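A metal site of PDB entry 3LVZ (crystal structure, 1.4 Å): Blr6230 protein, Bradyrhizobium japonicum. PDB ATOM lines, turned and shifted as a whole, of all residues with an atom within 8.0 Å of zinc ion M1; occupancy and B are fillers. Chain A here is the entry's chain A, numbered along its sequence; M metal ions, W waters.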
ATOM      1  N   PHE A  26       7.786   7.766  -9.072  1.00  0.00           N
ATOM      2  CA  PHE A  26       7.536   7.697  -7.652  1.00  0.00           C
ATOM      3  C   PHE A  26       6.051   7.208  -7.371  1.00  0.00           C
ATOM      4  O   PHE A  26       5.778   6.307  -6.550  1.00  0.00           O
ATOM      5  CB  PHE A  26       7.806   9.092  -7.052  1.00  0.00           C
ATOM      6  CG  PHE A  26       7.557   9.156  -5.556  1.00  0.00           C
ATOM      7  CD1 PHE A  26       8.577   8.861  -4.659  1.00  0.00           C
ATOM      8  CD2 PHE A  26       6.289   9.474  -5.071  1.00  0.00           C
ATOM      9  CE1 PHE A  26       8.336   8.920  -3.285  1.00  0.00           C
ATOM     10  CE2 PHE A  26       6.039   9.519  -3.720  1.00  0.00           C
ATOM     11  CZ  PHE A  26       7.040   9.260  -2.838  1.00  0.00           C
ATOM     12  N   TRP A  34       4.587  -0.622  -3.089  1.00  0.00           N
ATOM     13  CA  TRP A  34       4.288   0.053  -1.831  1.00  0.00           C
ATOM     14  C   TRP A  34       2.942  -0.267  -1.296  1.00  0.00           C
ATOM     15  O   TRP A  34       2.717  -0.099  -0.080  1.00  0.00           O
ATOM     16  CB  TRP A  34       4.396   1.564  -1.959  1.00  0.00           C
ATOM     17  CG  TRP A  34       5.777   2.090  -2.059  1.00  0.00           C
ATOM     18  CD1 TRP A  34       6.966   1.383  -2.148  1.00  0.00           C
ATOM     19  CD2 TRP A  34       6.162   3.468  -2.038  1.00  0.00           C
ATOM     20  NE1 TRP A  34       8.016   2.221  -2.190  1.00  0.00           N
ATOM     21  CE2 TRP A  34       7.569   3.514  -2.100  1.00  0.00           C
ATOM     22  CE3 TRP A  34       5.443   4.659  -2.018  1.00  0.00           C
ATOM     23  CZ2 TRP A  34       8.286   4.714  -2.114  1.00  0.00           C
ATOM     24  CZ3 TRP A  34       6.207   5.867  -2.072  1.00  0.00           C
ATOM     25  CH2 TRP A  34       7.568   5.840  -2.064  1.00  0.00           C
ATOM     26  N   GLY A  54       6.502  -2.909   0.340  1.00  0.00           N
ATOM     27  CA  GLY A  54       7.394  -1.870  -0.015  1.00  0.00           C
ATOM     28  C   GLY A  54       7.523  -0.638   0.928  1.00  0.00           C
ATOM     29  O   GLY A  54       8.378   0.165   0.703  1.00  0.00           O
ATOM     30  N   ILE A  55       6.738  -0.583   2.033  1.00  0.00           N
ATOM     31  CA  ILE A  55       6.749   0.454   3.077  1.00  0.00           C
ATOM     32  C   ILE A  55       6.752  -0.309   4.361  1.00  0.00           C
ATOM     33  O   ILE A  55       5.899  -1.113   4.638  1.00  0.00           O
ATOM     34  CB  ILE A  55       5.610   1.413   2.978  1.00  0.00           C
ATOM     35  CG1 ILE A  55       5.729   2.270   1.695  1.00  0.00           C
ATOM     36  CG2 ILE A  55       5.647   2.364   4.160  1.00  0.00           C
ATOM     37  CD1 ILE A  55       4.435   3.060   1.410  1.00  0.00           C
ATOM     38  N   ALA A  56       7.763  -0.016   5.174  1.00  0.00           N
ATOM     39  CA  ALA A  56       7.868  -0.685   6.486  1.00  0.00           C
ATOM     40  C   ALA A  56       7.216   0.086   7.576  1.00  0.00           C
ATOM     41  O   ALA A  56       7.389   1.338   7.726  1.00  0.00           O
ATOM     42  CB  ALA A  56       9.287  -0.852   6.825  1.00  0.00           C
ATOM     43  N   ASP A  70       5.612   4.821  12.322  1.00  0.00           N
ATOM     44  CA  ASP A  70       5.172   5.232  10.963  1.00  0.00           C
ATOM     45  C   ASP A  70       3.796   4.643  10.579  1.00  0.00           C
ATOM     46  O   ASP A  70       3.149   3.850  11.257  1.00  0.00           O
ATOM     47  CB  ASP A  70       6.277   4.927   9.933  1.00  0.00           C
ATOM     48  CG  ASP A  70       7.482   5.843  10.055  1.00  0.00           C
ATOM     49  OD1 ASP A  70       7.349   7.043  10.500  1.00  0.00           O
ATOM     50  OD2 ASP A  70       8.600   5.336   9.715  1.00  0.00           O
ATOM     51  N   MET A  73       1.097   4.822   2.790  1.00  0.00           N
ATOM     52  CA  MET A  73       0.387   5.779   1.932  1.00  0.00           C
ATOM     53  C   MET A  73      -0.967   6.101   2.498  1.00  0.00           C
ATOM     54  O   MET A  73      -1.554   5.253   3.170  1.00  0.00           O
ATOM     55  CB  MET A  73       0.264   5.262   0.520  1.00  0.00           C
ATOM     56  CG  MET A  73       1.597   5.139  -0.202  1.00  0.00           C
ATOM     57  SD  MET A  73       2.272   6.750  -0.683  1.00  0.00           S
ATOM     58  CE  MET A  73       1.164   7.296  -1.967  1.00  0.00           C
ATOM     59  N   THR A 100       9.585   8.548  11.570  1.00  0.00           N
ATOM     60  CA  THR A 100      10.951   8.621  11.056  1.00  0.00           C
ATOM     61  C   THR A 100      11.096   9.945  10.263  1.00  0.00           C
ATOM     62  O   THR A 100      11.960  10.768  10.525  1.00  0.00           O
ATOM     63  CB  THR A 100      11.332   7.461  10.138  1.00  0.00           C
ATOM     64  OG1 THR A 100      10.343   7.248   9.146  1.00  0.00           O
ATOM     65  CG2 THR A 100      11.668   6.259  10.929  1.00  0.00           C
ATOM     66  N   HIS A 101      10.288  10.167   9.252  1.00  0.00           N
ATOM     67  CA  HIS A 101      10.295  11.395   8.516  1.00  0.00           C
ATOM     68  C   HIS A 101       9.000  11.718   7.819  1.00  0.00           C
ATOM     69  O   HIS A 101       8.215  10.783   7.533  1.00  0.00           O
ATOM     70  CB  HIS A 101      11.443  11.423   7.503  1.00  0.00           C
ATOM     71  CG  HIS A 101      11.268  10.606   6.258  1.00  0.00           C
ATOM     72  ND1 HIS A 101      11.634   9.311   6.199  1.00  0.00           N
ATOM     73  CD2 HIS A 101      10.686  10.884   5.068  1.00  0.00           C
ATOM     74  CE1 HIS A 101      11.360   8.859   4.978  1.00  0.00           C
ATOM     75  NE2 HIS A 101      10.743   9.773   4.277  1.00  0.00           N
ATOM     76  N   HIS A 103       7.199  12.376   5.035  1.00  0.00           N
ATOM     77  CA  HIS A 103       6.721  12.242   3.656  1.00  0.00           C
ATOM     78  C   HIS A 103       5.483  11.366   3.609  1.00  0.00           C
ATOM     79  O   HIS A 103       5.339  10.480   4.494  1.00  0.00           O
ATOM     80  CB  HIS A 103       7.779  11.623   2.773  1.00  0.00           C
ATOM     81  CG  HIS A 103       8.976  12.460   2.520  1.00  0.00           C
ATOM     82  ND1 HIS A 103      10.194  11.927   2.132  1.00  0.00           N
ATOM     83  CD2 HIS A 103       9.103  13.805   2.527  1.00  0.00           C
ATOM     84  CE1 HIS A 103      11.015  12.941   1.914  1.00  0.00           C
ATOM     85  NE2 HIS A 103      10.408  14.087   2.188  1.00  0.00           N
ATOM     86  N   LEU A 104       4.607  11.538   2.611  1.00  0.00           N
ATOM     87  CA  LEU A 104       3.298  10.909   2.572  1.00  0.00           C
ATOM     88  C   LEU A 104       3.331   9.409   2.633  1.00  0.00           C
ATOM     89  O   LEU A 104       2.378   8.792   3.095  1.00  0.00           O
ATOM     90  CB  LEU A 104       2.505  11.332   1.374  1.00  0.00           C
ATOM     91  CG  LEU A 104       2.738  10.678   0.058  1.00  0.00           C
ATOM     92  CD1 LEU A 104       1.574  10.999  -0.843  1.00  0.00           C
ATOM     93  CD2 LEU A 104       4.035  11.127  -0.579  1.00  0.00           C
ATOM     94  N   ASP A 105       4.407   8.776   2.177  1.00  0.00           N
ATOM     95  CA  ASP A 105       4.437   7.298   2.216  1.00  0.00           C
ATOM     96  C   ASP A 105       4.688   6.735   3.607  1.00  0.00           C
ATOM     97  O   ASP A 105       4.600   5.521   3.819  1.00  0.00           O
ATOM     98  CB  ASP A 105       5.493   6.758   1.190  1.00  0.00           C
ATOM     99  CG  ASP A 105       6.850   7.323   1.302  1.00  0.00           C
ATOM    100  OD1 ASP A 105       7.059   8.561   1.543  1.00  0.00           O
ATOM    101  OD2 ASP A 105       7.850   6.514   1.163  1.00  0.00           O
ATOM    102  N   HIS A 106       4.958   7.622   4.558  1.00  0.00           N
ATOM    103  CA  HIS A 106       5.168   7.285   5.984  1.00  0.00           C
ATOM    104  C   HIS A 106       4.171   7.947   6.914  1.00  0.00           C
ATOM    105  O   HIS A 106       3.968   7.452   8.019  1.00  0.00           O
ATOM    106  CB  HIS A 106       6.579   7.541   6.454  1.00  0.00           C
ATOM    107  CG  HIS A 106       7.584   6.985   5.517  1.00  0.00           C
ATOM    108  ND1 HIS A 106       7.718   5.618   5.338  1.00  0.00           N
ATOM    109  CD2 HIS A 106       8.352   7.579   4.566  1.00  0.00           C
ATOM    110  CE1 HIS A 106       8.592   5.408   4.355  1.00  0.00           C
ATOM    111  NE2 HIS A 106       9.003   6.596   3.873  1.00  0.00           N
ATOM    112  N   HIS A 177      17.282  13.581   4.195  1.00  0.00           N
ATOM    113  CA  HIS A 177      16.097  13.121   3.417  1.00  0.00           C
ATOM    114  C   HIS A 177      14.884  13.959   3.741  1.00  0.00           C
ATOM    115  O   HIS A 177      14.041  14.221   2.867  1.00  0.00           O
ATOM    116  CB  HIS A 177      15.883  11.649   3.675  1.00  0.00           C
ATOM    117  CG  HIS A 177      14.762  11.099   2.849  1.00  0.00           C
ATOM    118  ND1 HIS A 177      14.912  10.577   1.598  1.00  0.00           N
ATOM    119  CD2 HIS A 177      13.465  10.882   3.182  1.00  0.00           C
ATOM    120  CE1 HIS A 177      13.724  10.176   1.150  1.00  0.00           C
ATOM    121  NE2 HIS A 177      12.824  10.379   2.095  1.00  0.00           N
ATOM    122  N   CYS A 201      16.103   6.607   9.606  1.00  0.00           N
ATOM    123  CA  CYS A 201      15.050   7.405   9.051  1.00  0.00           C
ATOM    124  C   CYS A 201      14.886   7.490   7.569  1.00  0.00           C
ATOM    125  O   CYS A 201      13.852   7.904   7.135  1.00  0.00           O
ATOM    126  CB  CYS A 201      15.082   8.810   9.675  1.00  0.00           C
ATOM    127  SG  CYS A 201      16.290   9.867   8.955  1.00  0.00           S
ATOM    128  N   SER A 202      15.916   7.171   6.871  1.00  0.00           N
ATOM    129  CA  SER A 202      16.126   7.247   5.409  1.00  0.00           C
ATOM    130  C   SER A 202      17.241   8.240   5.067  1.00  0.00           C
ATOM    131  O   SER A 202      17.312   9.313   5.694  1.00  0.00           O
ATOM    132  CB  SER A 202      14.905   7.615   4.588  1.00  0.00           C
ATOM    133  OG  SER A 202      15.364   7.785   3.262  1.00  0.00           O
ATOM    134  N   THR A 204      18.190   8.413   1.421  1.00  0.00           N
ATOM    135  CA  THR A 204      18.163   8.463   0.004  1.00  0.00           C
ATOM    136  C   THR A 204      17.942   9.847  -0.498  1.00  0.00           C
ATOM    137  O   THR A 204      17.396  10.711   0.219  1.00  0.00           O
ATOM    138  CB  THR A 204      17.028   7.584  -0.575  1.00  0.00           C
ATOM    139  OG1 THR A 204      15.804   8.072  -0.044  1.00  0.00           O
ATOM    140  CG2 THR A 204      17.237   6.074  -0.140  1.00  0.00           C
ATOM    141  N   ALA A 206      16.234  10.482  -3.476  1.00  0.00           N
ATOM    142  CA  ALA A 206      14.853  10.338  -3.894  1.00  0.00           C
ATOM    143  C   ALA A 206      14.425  11.588  -4.635  1.00  0.00           C
ATOM    144  O   ALA A 206      15.071  11.983  -5.672  1.00  0.00           O
ATOM    145  CB  ALA A 206      13.979   9.979  -2.645  1.00  0.00           C
ATOM    146  N   PRO A 241      12.456   2.720   6.973  1.00  0.00           N
ATOM    147  CA  PRO A 241      11.053   2.937   6.597  1.00  0.00           C
ATOM    148  C   PRO A 241      10.612   2.279   5.269  1.00  0.00           C
ATOM    149  O   PRO A 241       9.404   2.300   4.938  1.00  0.00           O
ATOM    150  CB  PRO A 241      10.989   4.478   6.602  1.00  0.00           C
ATOM    151  CG  PRO A 241      12.329   4.961   6.491  1.00  0.00           C
ATOM    152  CD  PRO A 241      13.319   3.925   6.840  1.00  0.00           C
ATOM    153  N   HIS A 242      11.524   1.626   4.565  1.00  0.00           N
ATOM    154  CA  HIS A 242      11.260   0.727   3.472  1.00  0.00           C
ATOM    155  C   HIS A 242      12.044  -0.516   3.693  1.00  0.00           C
ATOM    156  O   HIS A 242      13.187  -0.483   4.163  1.00  0.00           O
ATOM    157  CB  HIS A 242      11.683   1.448   2.148  1.00  0.00           C
ATOM    158  CG  HIS A 242      10.866   2.670   1.856  1.00  0.00           C
ATOM    159  ND1 HIS A 242       9.624   2.617   1.227  1.00  0.00           N
ATOM    160  CD2 HIS A 242      11.161   3.980   2.038  1.00  0.00           C
ATOM    161  CE1 HIS A 242       9.167   3.864   1.097  1.00  0.00           C
ATOM    162  NE2 HIS A 242      10.077   4.706   1.557  1.00  0.00           N
HETATM  163 ZN    ZN M   1       9.744   6.696   1.946  1.00  0.00          ZN
HETATM  164 ZN    ZN M   2      10.835   9.956   2.231  1.00  0.00          ZN
HETATM  165  O   HOH W   1      12.214   6.998   2.371  1.00  0.00           O
HETATM  166  O   HOH W   2       9.741   8.651   1.305  1.00  0.00           O
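A ring nitrogen (ND1) of His 242 sits at hydrogen-bond distance from the backbone carbonyl oxygen (O) of Gly 54 (2.8 Å). A ring nitrogen (ND1) of His 101 sits at hydrogen-bond distance from the backbone carbonyl oxygen (O) of Cys 201 (2.8 Å).
NE2 of His 101 touches zinc ion M1 (3.99 Å). The nearest printed residue that does not touch zinc ion M1 is Trp 34 (4.6 Å).
Zinc ion M1 is bound by a ring nitrogen (NE2) of His 242, 2.1 Å away. Zinc ion M1 is bound by OD2 of Asp 105, at 2.1 Å. Water W2 binds zinc ion M1 (2.1 Å). NE2 of His 106 binds zinc ion M1, 2.1 Å away. Water W1 is bound to zinc ion M1 (2.5 Å). Zinc ion M1 has five donor atoms within binding distance.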
